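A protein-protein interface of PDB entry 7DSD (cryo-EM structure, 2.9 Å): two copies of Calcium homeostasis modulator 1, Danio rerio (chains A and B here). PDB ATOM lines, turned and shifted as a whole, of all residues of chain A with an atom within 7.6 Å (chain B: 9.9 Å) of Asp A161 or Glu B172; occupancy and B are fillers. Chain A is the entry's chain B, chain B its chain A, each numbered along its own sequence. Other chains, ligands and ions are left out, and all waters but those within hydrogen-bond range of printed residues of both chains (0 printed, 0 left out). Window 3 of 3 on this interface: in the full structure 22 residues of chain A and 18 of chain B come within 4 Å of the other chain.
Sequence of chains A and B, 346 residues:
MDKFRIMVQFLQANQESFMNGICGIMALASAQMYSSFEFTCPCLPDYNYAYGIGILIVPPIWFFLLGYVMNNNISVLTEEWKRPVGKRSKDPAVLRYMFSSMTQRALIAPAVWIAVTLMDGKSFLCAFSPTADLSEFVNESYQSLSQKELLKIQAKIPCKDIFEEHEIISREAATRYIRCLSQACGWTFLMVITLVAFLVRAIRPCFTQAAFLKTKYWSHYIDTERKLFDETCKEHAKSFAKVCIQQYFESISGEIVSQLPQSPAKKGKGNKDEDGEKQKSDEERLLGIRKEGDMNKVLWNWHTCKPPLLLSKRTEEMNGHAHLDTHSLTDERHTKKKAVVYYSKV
Among the printed residues, merely in contact across the chains: Ile A162 with Arg B176 (3.7 Å), Thr A40 with Arg B176 (3.8 Å) and Asp A161 with Glu B172 (3.9 Å).
Of chain A, only Asp A161 comes within 4 Å of Glu B172. Of the printed residues of chain B, Cys A41 touches Arg B176 (2.9 Å). Printed residues of chain B within 4 Å of Cys A159: Arg B176. Printed residues of chain B within 4 Å of Thr A40: Arg B176 and Cys B180. Printed residues of chain A within 4 Å of Arg B176: Thr A40, Cys A41, Cys A159 and Ile A162. Of the printed residues of chain B, Pro A42 touches Cys B180.
The backbone carbonyl oxygen (O) of Cys A41 sits at hydrogen-bond distance from the guanidinium group (NE) of Arg B176, at 2.9 Å. NE of Arg B176 lies within hydrogen-bond range of SG of Cys A159, 3.1 Å away. The side-chain sulfur of Cys B180 sits at hydrogen-bond distance from the backbone carbonyl oxygen of Thr A40 (3.1 Å). N of Pro A42 lies close to SG of Cys B180 (3.7 Å).
The guanidinium group (NH1) of Arg B171 is in salt-bridge range of the side-chain carboxylate (OE1) of Glu B172 (3.5 Å). OE2 of Glu B172 is in salt-bridge range of NH2 of Arg B176 (3.3 Å). The side-chain sulfur (SG) of Cys B180 lies within hydrogen-bond range of the backbone carbonyl oxygen (O) of Arg B176 (3.1 Å).
Of the 13 printed residues of chain A, 6 touch a printed residue of chain B. Printed residues of chain A that touch a printed residue of chain B: Thr A40, Cys A41, Pro A42, Cys A159, Asp A161 and Ile A162. Hydrophobic or aromatic side chains of chain A that line the printed part of chain B: Pro A42 and Ile A162. Of the 23 printed residues of chain B, 3 touch a printed residue of chain A. Along chain B the printed residues that touch a printed residue of chain A span positions 172 to 180. Among the printed residues, 7 pairs touch across the chains. Among the printed residues, no Asp or Glu carboxylate lies within 4 Å of a Lys or Arg side-chain nitrogen of the other chain.
7 positions are printed for both chains. Of the 7 pairs that touch across the chains among the printed residues, none has its exchanged pair printed and touching as well.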
ATOM      1  N   THR A  40      -7.193  20.022  11.293  1.00  0.00           N
ATOM      2  CA  THR A  40      -6.292  20.457  10.226  1.00  0.00           C
ATOM      3  C   THR A  40      -6.418  21.969  10.067  1.00  0.00           C
ATOM      4  O   THR A  40      -7.355  22.453   9.432  1.00  0.00           O
ATOM      5  CB  THR A  40      -6.606  19.741   8.921  1.00  0.00           C
ATOM      6  OG1 THR A  40      -5.583  20.029   7.963  1.00  0.00           O
ATOM      7  CG2 THR A  40      -7.941  20.200   8.380  1.00  0.00           C
ATOM      8  N   CYS A  41      -5.479  22.702  10.637  1.00  0.00           N
ATOM      9  CA  CYS A  41      -5.500  24.152  10.519  1.00  0.00           C
ATOM     10  C   CYS A  41      -5.140  24.540   9.093  1.00  0.00           C
ATOM     11  O   CYS A  41      -4.164  24.012   8.549  1.00  0.00           O
ATOM     12  CB  CYS A  41      -4.525  24.771  11.513  1.00  0.00           C
ATOM     13  SG  CYS A  41      -4.645  26.561  11.697  1.00  0.00           S
ATOM     14  N   PRO A  42      -5.893  25.430   8.446  1.00  0.00           N
ATOM     15  CA  PRO A  42      -5.558  25.799   7.065  1.00  0.00           C
ATOM     16  C   PRO A  42      -4.254  26.554   6.943  1.00  0.00           C
ATOM     17  O   PRO A  42      -3.667  26.569   5.855  1.00  0.00           O
ATOM     18  CB  PRO A  42      -6.749  26.661   6.634  1.00  0.00           C
ATOM     19  CG  PRO A  42      -7.295  27.192   7.897  1.00  0.00           C
ATOM     20  CD  PRO A  42      -7.096  26.126   8.925  1.00  0.00           C
ATOM     21  N   LYS A 156       1.570  30.420   9.765  1.00  0.00           N
ATOM     22  CA  LYS A 156       2.066  29.072   9.516  1.00  0.00           C
ATOM     23  C   LYS A 156       2.607  28.384  10.762  1.00  0.00           C
ATOM     24  O   LYS A 156       3.218  27.317  10.635  1.00  0.00           O
ATOM     25  CB  LYS A 156       3.170  29.105   8.457  1.00  0.00           C
ATOM     26  CG  LYS A 156       2.835  29.908   7.224  1.00  0.00           C
ATOM     27  CD  LYS A 156       4.036  29.991   6.305  1.00  0.00           C
ATOM     28  CE  LYS A 156       3.756  30.873   5.106  1.00  0.00           C
ATOM     29  NZ  LYS A 156       4.967  31.037   4.258  1.00  0.00           N
ATOM     30  N   ILE A 157       2.412  28.954  11.949  1.00  0.00           N
ATOM     31  CA  ILE A 157       2.985  28.359  13.157  1.00  0.00           C
ATOM     32  C   ILE A 157       2.349  27.018  13.509  1.00  0.00           C
ATOM     33  O   ILE A 157       3.089  26.080  13.846  1.00  0.00           O
ATOM     34  CB  ILE A 157       2.932  29.367  14.318  1.00  0.00           C
ATOM     35  CG1 ILE A 157       4.024  30.420  14.151  1.00  0.00           C
ATOM     36  CG2 ILE A 157       3.083  28.662  15.647  1.00  0.00           C
ATOM     37  CD1 ILE A 157       4.116  31.381  15.301  1.00  0.00           C
ATOM     38  N   PRO A 158       1.022  26.847  13.461  1.00  0.00           N
ATOM     39  CA  PRO A 158       0.453  25.533  13.794  1.00  0.00           C
ATOM     40  C   PRO A 158       0.777  24.432  12.796  1.00  0.00           C
ATOM     41  O   PRO A 158       0.409  23.279  13.042  1.00  0.00           O
ATOM     42  CB  PRO A 158      -1.057  25.806  13.835  1.00  0.00           C
ATOM     43  CG  PRO A 158      -1.244  27.032  13.048  1.00  0.00           C
ATOM     44  CD  PRO A 158      -0.037  27.857  13.304  1.00  0.00           C
ATOM     45  N   CYS A 159       1.447  24.731  11.689  1.00  0.00           N
ATOM     46  CA  CYS A 159       1.769  23.741  10.665  1.00  0.00           C
ATOM     47  C   CYS A 159       3.265  23.456  10.720  1.00  0.00           C
ATOM     48  O   CYS A 159       4.081  24.314  10.378  1.00  0.00           O
ATOM     49  CB  CYS A 159       1.350  24.233   9.283  1.00  0.00           C
ATOM     50  SG  CYS A 159      -0.429  24.207   8.984  1.00  0.00           S
ATOM     51  N   LYS A 160       3.625  22.247  11.155  1.00  0.00           N
ATOM     52  CA  LYS A 160       5.033  21.871  11.195  1.00  0.00           C
ATOM     53  C   LYS A 160       5.608  21.754   9.791  1.00  0.00           C
ATOM     54  O   LYS A 160       6.753  22.149   9.542  1.00  0.00           O
ATOM     55  CB  LYS A 160       5.209  20.554  11.947  1.00  0.00           C
ATOM     56  CG  LYS A 160       4.687  20.561  13.365  1.00  0.00           C
ATOM     57  CD  LYS A 160       4.903  19.206  14.012  1.00  0.00           C
ATOM     58  CE  LYS A 160       4.327  19.164  15.413  1.00  0.00           C
ATOM     59  NZ  LYS A 160       4.519  17.829  16.043  1.00  0.00           N
ATOM     60  N   ASP A 161       4.826  21.210   8.860  1.00  0.00           N
ATOM     61  CA  ASP A 161       5.316  20.938   7.515  1.00  0.00           C
ATOM     62  C   ASP A 161       5.451  22.191   6.665  1.00  0.00           C
ATOM     63  O   ASP A 161       6.270  22.202   5.741  1.00  0.00           O
ATOM     64  CB  ASP A 161       4.385  19.951   6.818  1.00  0.00           C
ATOM     65  CG  ASP A 161       4.487  18.556   7.390  1.00  0.00           C
ATOM     66  OD1 ASP A 161       5.463  18.284   8.119  1.00  0.00           O
ATOM     67  OD2 ASP A 161       3.588  17.733   7.120  1.00  0.00           O
ATOM     68  N   ILE A 162       4.675  23.233   6.944  1.00  0.00           N
ATOM     69  CA  ILE A 162       4.697  24.439   6.139  1.00  0.00           C
ATOM     70  C   ILE A 162       5.655  25.490   6.686  1.00  0.00           C
ATOM     71  O   ILE A 162       6.208  26.271   5.903  1.00  0.00           O
ATOM     72  CB  ILE A 162       3.275  25.019   6.004  1.00  0.00           C
ATOM     73  CG1 ILE A 162       2.281  23.899   5.714  1.00  0.00           C
ATOM     74  CG2 ILE A 162       3.226  26.056   4.904  1.00  0.00           C
ATOM     75  CD1 ILE A 162       0.864  24.380   5.578  1.00  0.00           C
ATOM     76  N   PHE A 163       5.873  25.533   7.997  1.00  0.00           N
ATOM     77  CA  PHE A 163       6.723  26.554   8.597  1.00  0.00           C
ATOM     78  C   PHE A 163       8.167  26.335   8.166  1.00  0.00           C
ATOM     79  O   PHE A 163       8.752  25.282   8.438  1.00  0.00           O
ATOM     80  CB  PHE A 163       6.594  26.519  10.115  1.00  0.00           C
ATOM     81  CG  PHE A 163       7.195  27.708  10.794  1.00  0.00           C
ATOM     82  CD1 PHE A 163       6.482  28.883  10.912  1.00  0.00           C
ATOM     83  CD2 PHE A 163       8.475  27.653  11.309  1.00  0.00           C
ATOM     84  CE1 PHE A 163       7.032  29.981  11.532  1.00  0.00           C
ATOM     85  CE2 PHE A 163       9.027  28.749  11.930  1.00  0.00           C
ATOM     86  CZ  PHE A 163       8.305  29.913  12.042  1.00  0.00           C
ATOM     87  N   GLU A 164       8.740  27.321   7.487  1.00  0.00           N
ATOM     88  CA  GLU A 164      10.119  27.271   7.020  1.00  0.00           C
ATOM     89  C   GLU A 164      10.826  28.594   7.279  1.00  0.00           C
ATOM     90  O   GLU A 164      11.638  29.056   6.475  1.00  0.00           O
ATOM     91  CB  GLU A 164      10.179  26.909   5.538  1.00  0.00           C
ATOM     92  CG  GLU A 164       9.685  25.509   5.221  1.00  0.00           C
ATOM     93  CD  GLU A 164       9.716  25.203   3.739  1.00  0.00           C
ATOM     94  OE1 GLU A 164      10.133  26.085   2.959  1.00  0.00           O
ATOM     95  OE2 GLU A 164       9.323  24.082   3.351  1.00  0.00           O
ATOM     96  N   ARG A 171       9.272  28.372  16.518  1.00  0.00           N
ATOM     97  CA  ARG A 171       7.912  27.854  16.411  1.00  0.00           C
ATOM     98  C   ARG A 171       7.483  27.141  17.686  1.00  0.00           C
ATOM     99  O   ARG A 171       6.349  27.315  18.152  1.00  0.00           O
ATOM    100  CB  ARG A 171       7.805  26.910  15.219  1.00  0.00           C
ATOM    101  CG  ARG A 171       6.393  26.473  14.909  1.00  0.00           C
ATOM    102  CD  ARG A 171       6.386  25.335  13.917  1.00  0.00           C
ATOM    103  NE  ARG A 171       6.953  24.130  14.500  1.00  0.00           N
ATOM    104  CZ  ARG A 171       6.255  23.258  15.215  1.00  0.00           C
ATOM    105  NH1 ARG A 171       6.846  22.183  15.715  1.00  0.00           N
ATOM    106  NH2 ARG A 171       4.964  23.462  15.428  1.00  0.00           N
ATOM    107  N   LEU B 125     -10.418  15.829  -1.720  1.00  0.00           N
ATOM    108  CA  LEU B 125      -9.059  16.090  -2.176  1.00  0.00           C
ATOM    109  C   LEU B 125      -8.768  15.356  -3.474  1.00  0.00           C
ATOM    110  O   LEU B 125      -8.106  15.891  -4.367  1.00  0.00           O
ATOM    111  CB  LEU B 125      -8.064  15.683  -1.092  1.00  0.00           C
ATOM    112  CG  LEU B 125      -6.589  15.876  -1.419  1.00  0.00           C
ATOM    113  CD1 LEU B 125      -6.301  17.331  -1.708  1.00  0.00           C
ATOM    114  CD2 LEU B 125      -5.741  15.373  -0.272  1.00  0.00           C
ATOM    115  N   LEU B 134      -6.005  26.918  -7.535  1.00  0.00           N
ATOM    116  CA  LEU B 134      -4.915  27.107  -6.585  1.00  0.00           C
ATOM    117  C   LEU B 134      -3.940  28.084  -7.227  1.00  0.00           C
ATOM    118  O   LEU B 134      -2.957  27.688  -7.853  1.00  0.00           O
ATOM    119  CB  LEU B 134      -4.252  25.785  -6.246  1.00  0.00           C
ATOM    120  CG  LEU B 134      -5.208  24.656  -5.864  1.00  0.00           C
ATOM    121  CD1 LEU B 134      -4.453  23.366  -5.631  1.00  0.00           C
ATOM    122  CD2 LEU B 134      -6.005  25.035  -4.635  1.00  0.00           C
ATOM    123  N   PHE B 137      -1.124  29.172  -3.995  1.00  0.00           N
ATOM    124  CA  PHE B 137      -0.072  28.233  -3.641  1.00  0.00           C
ATOM    125  C   PHE B 137       0.941  28.032  -4.754  1.00  0.00           C
ATOM    126  O   PHE B 137       2.068  27.605  -4.483  1.00  0.00           O
ATOM    127  CB  PHE B 137      -0.684  26.886  -3.262  1.00  0.00           C
ATOM    128  CG  PHE B 137      -1.835  26.998  -2.312  1.00  0.00           C
ATOM    129  CD1 PHE B 137      -1.614  27.146  -0.959  1.00  0.00           C
ATOM    130  CD2 PHE B 137      -3.134  26.963  -2.772  1.00  0.00           C
ATOM    131  CE1 PHE B 137      -2.669  27.251  -0.081  1.00  0.00           C
ATOM    132  CE2 PHE B 137      -4.193  27.070  -1.898  1.00  0.00           C
ATOM    133  CZ  PHE B 137      -3.960  27.214  -0.552  1.00  0.00           C
ATOM    134  N   LYS B 156      -1.688  15.253  -9.243  1.00  0.00           N
ATOM    135  CA  LYS B 156      -0.836  14.428  -8.397  1.00  0.00           C
ATOM    136  C   LYS B 156      -0.753  14.916  -6.957  1.00  0.00           C
ATOM    137  O   LYS B 156       0.080  14.406  -6.202  1.00  0.00           O
ATOM    138  CB  LYS B 156       0.579  14.368  -8.976  1.00  0.00           C
ATOM    139  CG  LYS B 156       0.643  14.062 -10.451  1.00  0.00           C
ATOM    140  CD  LYS B 156       2.070  14.159 -10.950  1.00  0.00           C
ATOM    141  CE  LYS B 156       2.147  13.951 -12.448  1.00  0.00           C
ATOM    142  NZ  LYS B 156       3.533  14.150 -12.952  1.00  0.00           N
ATOM    143  N   ILE B 157      -1.575  15.884  -6.557  1.00  0.00           N
ATOM    144  CA  ILE B 157      -1.469  16.430  -5.203  1.00  0.00           C
ATOM    145  C   ILE B 157      -1.865  15.420  -4.131  1.00  0.00           C
ATOM    146  O   ILE B 157      -1.153  15.317  -3.119  1.00  0.00           O
ATOM    147  CB  ILE B 157      -2.259  17.746  -5.101  1.00  0.00           C
ATOM    148  CG1 ILE B 157      -1.483  18.878  -5.769  1.00  0.00           C
ATOM    149  CG2 ILE B 157      -2.548  18.088  -3.657  1.00  0.00           C
ATOM    150  CD1 ILE B 157      -2.129  20.225  -5.616  1.00  0.00           C
ATOM    151  N   PRO B 158      -2.956  14.657  -4.267  1.00  0.00           N
ATOM    152  CA  PRO B 158      -3.291  13.685  -3.216  1.00  0.00           C
ATOM    153  C   PRO B 158      -2.317  12.524  -3.093  1.00  0.00           C
ATOM    154  O   PRO B 158      -2.476  11.707  -2.181  1.00  0.00           O
ATOM    155  CB  PRO B 158      -4.683  13.188  -3.629  1.00  0.00           C
ATOM    156  CG  PRO B 158      -4.786  13.491  -5.063  1.00  0.00           C
ATOM    157  CD  PRO B 158      -4.041  14.759  -5.256  1.00  0.00           C
ATOM    158  N   CYS B 159      -1.319  12.416  -3.962  1.00  0.00           N
ATOM    159  CA  CYS B 159      -0.360  11.313  -3.936  1.00  0.00           C
ATOM    160  C   CYS B 159       0.980  11.850  -3.449  1.00  0.00           C
ATOM    161  O   CYS B 159       1.639  12.622  -4.149  1.00  0.00           O
ATOM    162  CB  CYS B 159      -0.232  10.671  -5.314  1.00  0.00           C
ATOM    163  SG  CYS B 159      -1.639   9.655  -5.802  1.00  0.00           S
ATOM    164  N   LYS B 160       1.383  11.441  -2.244  1.00  0.00           N
ATOM    165  CA  LYS B 160       2.675  11.867  -1.719  1.00  0.00           C
ATOM    166  C   LYS B 160       3.818  11.263  -2.524  1.00  0.00           C
ATOM    167  O   LYS B 160       4.829  11.925  -2.781  1.00  0.00           O
ATOM    168  CB  LYS B 160       2.805  11.478  -0.248  1.00  0.00           C
ATOM    169  CG  LYS B 160       1.728  12.040   0.651  1.00  0.00           C
ATOM    170  CD  LYS B 160       1.946  11.585   2.080  1.00  0.00           C
ATOM    171  CE  LYS B 160       0.841  12.080   2.993  1.00  0.00           C
ATOM    172  NZ  LYS B 160       1.041  11.618   4.394  1.00  0.00           N
ATOM    173  N   PHE B 163       3.957  12.942  -6.361  1.00  0.00           N
ATOM    174  CA  PHE B 163       4.195  14.373  -6.508  1.00  0.00           C
ATOM    175  C   PHE B 163       5.688  14.655  -6.416  1.00  0.00           C
ATOM    176  O   PHE B 163       6.321  14.366  -5.397  1.00  0.00           O
ATOM    177  CB  PHE B 163       3.425  15.147  -5.446  1.00  0.00           C
ATOM    178  CG  PHE B 163       3.373  16.619  -5.697  1.00  0.00           C
ATOM    179  CD1 PHE B 163       2.429  17.152  -6.551  1.00  0.00           C
ATOM    180  CD2 PHE B 163       4.270  17.471  -5.086  1.00  0.00           C
ATOM    181  CE1 PHE B 163       2.379  18.506  -6.790  1.00  0.00           C
ATOM    182  CE2 PHE B 163       4.223  18.825  -5.321  1.00  0.00           C
ATOM    183  CZ  PHE B 163       3.277  19.342  -6.174  1.00  0.00           C
ATOM    184  N   GLU B 165       6.955  17.856  -7.860  1.00  0.00           N
ATOM    185  CA  GLU B 165       6.975  19.206  -8.409  1.00  0.00           C
ATOM    186  C   GLU B 165       6.964  20.228  -7.284  1.00  0.00           C
ATOM    187  O   GLU B 165       6.200  21.195  -7.292  1.00  0.00           O
ATOM    188  CB  GLU B 165       5.802  19.431  -9.354  1.00  0.00           C
ATOM    189  CG  GLU B 165       5.834  18.579 -10.614  1.00  0.00           C
ATOM    190  CD  GLU B 165       5.356  17.158 -10.385  1.00  0.00           C
ATOM    191  OE1 GLU B 165       5.055  16.803  -9.226  1.00  0.00           O
ATOM    192  OE2 GLU B 165       5.274  16.395 -11.370  1.00  0.00           O
ATOM    193  N   HIS B 166       7.826  20.018  -6.288  1.00  0.00           N
ATOM    194  CA  HIS B 166       7.871  20.911  -5.138  1.00  0.00           C
ATOM    195  C   HIS B 166       8.292  22.323  -5.513  1.00  0.00           C
ATOM    196  O   HIS B 166       8.002  23.261  -4.763  1.00  0.00           O
ATOM    197  CB  HIS B 166       8.819  20.353  -4.081  1.00  0.00           C
ATOM    198  CG  HIS B 166       8.425  19.005  -3.569  1.00  0.00           C
ATOM    199  ND1 HIS B 166       7.425  18.825  -2.639  1.00  0.00           N
ATOM    200  CD2 HIS B 166       8.900  17.770  -3.855  1.00  0.00           C
ATOM    201  CE1 HIS B 166       7.299  17.537  -2.374  1.00  0.00           C
ATOM    202  NE2 HIS B 166       8.181  16.875  -3.101  1.00  0.00           N
ATOM    203  N   ILE B 169       4.330  23.994  -6.774  1.00  0.00           N
ATOM    204  CA  ILE B 169       3.172  24.101  -5.896  1.00  0.00           C
ATOM    205  C   ILE B 169       3.502  23.451  -4.564  1.00  0.00           C
ATOM    206  O   ILE B 169       4.045  22.344  -4.517  1.00  0.00           O
ATOM    207  CB  ILE B 169       1.921  23.453  -6.525  1.00  0.00           C
ATOM    208  CG1 ILE B 169       1.339  24.356  -7.609  1.00  0.00           C
ATOM    209  CG2 ILE B 169       0.872  23.162  -5.471  1.00  0.00           C
ATOM    210  CD1 ILE B 169      -0.007  23.897  -8.107  1.00  0.00           C
ATOM    211  N   SER B 170       3.179  24.144  -3.477  1.00  0.00           N
ATOM    212  CA  SER B 170       3.272  23.564  -2.144  1.00  0.00           C
ATOM    213  C   SER B 170       2.150  22.546  -1.991  1.00  0.00           C
ATOM    214  O   SER B 170       0.970  22.904  -2.043  1.00  0.00           O
ATOM    215  CB  SER B 170       3.184  24.652  -1.081  1.00  0.00           C
ATOM    216  OG  SER B 170       3.240  24.094   0.219  1.00  0.00           O
ATOM    217  N   ARG B 171       2.512  21.276  -1.814  1.00  0.00           N
ATOM    218  CA  ARG B 171       1.497  20.227  -1.754  1.00  0.00           C
ATOM    219  C   ARG B 171       0.731  20.263  -0.439  1.00  0.00           C
ATOM    220  O   ARG B 171      -0.497  20.115  -0.424  1.00  0.00           O
ATOM    221  CB  ARG B 171       2.147  18.862  -1.948  1.00  0.00           C
ATOM    222  CG  ARG B 171       1.158  17.731  -2.097  1.00  0.00           C
ATOM    223  CD  ARG B 171       1.851  16.393  -2.001  1.00  0.00           C
ATOM    224  NE  ARG B 171       2.367  16.167  -0.659  1.00  0.00           N
ATOM    225  CZ  ARG B 171       1.650  15.652   0.329  1.00  0.00           C
ATOM    226  NH1 ARG B 171       2.193  15.480   1.525  1.00  0.00           N
ATOM    227  NH2 ARG B 171       0.389  15.307   0.121  1.00  0.00           N
ATOM    228  N   GLU B 172       1.438  20.463   0.675  1.00  0.00           N
ATOM    229  CA  GLU B 172       0.799  20.357   1.981  1.00  0.00           C
ATOM    230  C   GLU B 172      -0.187  21.494   2.213  1.00  0.00           C
ATOM    231  O   GLU B 172      -1.251  21.287   2.807  1.00  0.00           O
ATOM    232  CB  GLU B 172       1.857  20.328   3.078  1.00  0.00           C
ATOM    233  CG  GLU B 172       1.299  20.095   4.470  1.00  0.00           C
ATOM    234  CD  GLU B 172       0.719  18.704   4.649  1.00  0.00           C
ATOM    235  OE1 GLU B 172       1.083  17.795   3.873  1.00  0.00           O
ATOM    236  OE2 GLU B 172      -0.102  18.518   5.571  1.00  0.00           O
ATOM    237  N   ALA B 173       0.145  22.699   1.752  1.00  0.00           N
ATOM    238  CA  ALA B 173      -0.768  23.825   1.909  1.00  0.00           C
ATOM    239  C   ALA B 173      -2.087  23.565   1.195  1.00  0.00           C
ATOM    240  O   ALA B 173      -3.169  23.752   1.769  1.00  0.00           O
ATOM    241  CB  ALA B 173      -0.110  25.100   1.391  1.00  0.00           C
ATOM    242  N   ALA B 174      -2.016  23.129  -0.063  1.00  0.00           N
ATOM    243  CA  ALA B 174      -3.231  22.845  -0.818  1.00  0.00           C
ATOM    244  C   ALA B 174      -4.008  21.694  -0.198  1.00  0.00           C
ATOM    245  O   ALA B 174      -5.246  21.713  -0.164  1.00  0.00           O
ATOM    246  CB  ALA B 174      -2.882  22.537  -2.270  1.00  0.00           C
ATOM    247  N   THR B 175      -3.296  20.680   0.298  1.00  0.00           N
ATOM    248  CA  THR B 175      -3.961  19.572   0.971  1.00  0.00           C
ATOM    249  C   THR B 175      -4.767  20.062   2.168  1.00  0.00           C
ATOM    250  O   THR B 175      -5.942  19.708   2.326  1.00  0.00           O
ATOM    251  CB  THR B 175      -2.932  18.534   1.404  1.00  0.00           C
ATOM    252  OG1 THR B 175      -2.305  17.977   0.244  1.00  0.00           O
ATOM    253  CG2 THR B 175      -3.593  17.424   2.190  1.00  0.00           C
ATOM    254  N   ARG B 176      -4.151  20.883   3.020  1.00  0.00           N
ATOM    255  CA  ARG B 176      -4.858  21.395   4.190  1.00  0.00           C
ATOM    256  C   ARG B 176      -6.042  22.264   3.787  1.00  0.00           C
ATOM    257  O   ARG B 176      -7.112  22.189   4.399  1.00  0.00           O
ATOM    258  CB  ARG B 176      -3.900  22.177   5.082  1.00  0.00           C
ATOM    259  CG  ARG B 176      -2.741  21.356   5.593  1.00  0.00           C
ATOM    260  CD  ARG B 176      -1.884  22.154   6.543  1.00  0.00           C
ATOM    261  NE  ARG B 176      -2.240  21.900   7.933  1.00  0.00           N
ATOM    262  CZ  ARG B 176      -1.609  21.027   8.709  1.00  0.00           C
ATOM    263  NH1 ARG B 176      -1.993  20.852   9.965  1.00  0.00           N
ATOM    264  NH2 ARG B 176      -0.588  20.334   8.231  1.00  0.00           N
ATOM    265  N   TYR B 177      -5.868  23.092   2.758  1.00  0.00           N
ATOM    266  CA  TYR B 177      -6.958  23.937   2.280  1.00  0.00           C
ATOM    267  C   TYR B 177      -8.170  23.097   1.884  1.00  0.00           C
ATOM    268  O   TYR B 177      -9.298  23.330   2.349  1.00  0.00           O
ATOM    269  CB  TYR B 177      -6.460  24.768   1.102  1.00  0.00           C
ATOM    270  CG  TYR B 177      -7.458  25.735   0.529  1.00  0.00           C
ATOM    271  CD1 TYR B 177      -8.444  26.298   1.318  1.00  0.00           C
ATOM    272  CD2 TYR B 177      -7.412  26.085  -0.808  1.00  0.00           C
ATOM    273  CE1 TYR B 177      -9.355  27.186   0.789  1.00  0.00           C
ATOM    274  CE2 TYR B 177      -8.316  26.967  -1.345  1.00  0.00           C
ATOM    275  CZ  TYR B 177      -9.285  27.515  -0.544  1.00  0.00           C
ATOM    276  OH  TYR B 177     -10.190  28.398  -1.086  1.00  0.00           O
ATOM    277  N   ILE B 178      -7.951  22.101   1.026  1.00  0.00           N
ATOM    278  CA  ILE B 178      -9.076  21.318   0.537  1.00  0.00           C
ATOM    279  C   ILE B 178      -9.668  20.465   1.648  1.00  0.00           C
ATOM    280  O   ILE B 178     -10.884  20.235   1.683  1.00  0.00           O
ATOM    281  CB  ILE B 178      -8.647  20.471  -0.669  1.00  0.00           C
ATOM    282  CG1 ILE B 178      -8.083  21.376  -1.759  1.00  0.00           C
ATOM    283  CG2 ILE B 178      -9.821  19.696  -1.209  1.00  0.00           C
ATOM    284  CD1 ILE B 178      -7.610  20.633  -2.972  1.00  0.00           C
ATOM    285  N   ARG B 179      -8.845  20.009   2.593  1.00  0.00           N
ATOM    286  CA  ARG B 179      -9.386  19.238   3.706  1.00  0.00           C
ATOM    287  C   ARG B 179     -10.275  20.103   4.592  1.00  0.00           C
ATOM    288  O   ARG B 179     -11.307  19.636   5.091  1.00  0.00           O
ATOM    289  CB  ARG B 179      -8.249  18.623   4.511  1.00  0.00           C
ATOM    290  CG  ARG B 179      -7.501  17.530   3.783  1.00  0.00           C
ATOM    291  CD  ARG B 179      -6.346  17.024   4.622  1.00  0.00           C
ATOM    292  NE  ARG B 179      -6.806  16.394   5.853  1.00  0.00           N
ATOM    293  CZ  ARG B 179      -7.199  15.128   5.936  1.00  0.00           C
ATOM    294  NH1 ARG B 179      -7.601  14.631   7.099  1.00  0.00           N
ATOM    295  NH2 ARG B 179      -7.193  14.359   4.858  1.00  0.00           N
ATOM    296  N   CYS B 180      -9.895  21.368   4.795  1.00  0.00           N
ATOM    297  CA  CYS B 180     -10.756  22.281   5.539  1.00  0.00           C
ATOM    298  C   CYS B 180     -12.086  22.486   4.828  1.00  0.00           C
ATOM    299  O   CYS B 180     -13.147  22.485   5.466  1.00  0.00           O
ATOM    300  CB  CYS B 180     -10.055  23.622   5.744  1.00  0.00           C
ATOM    301  SG  CYS B 180      -8.585  23.539   6.773  1.00  0.00           S
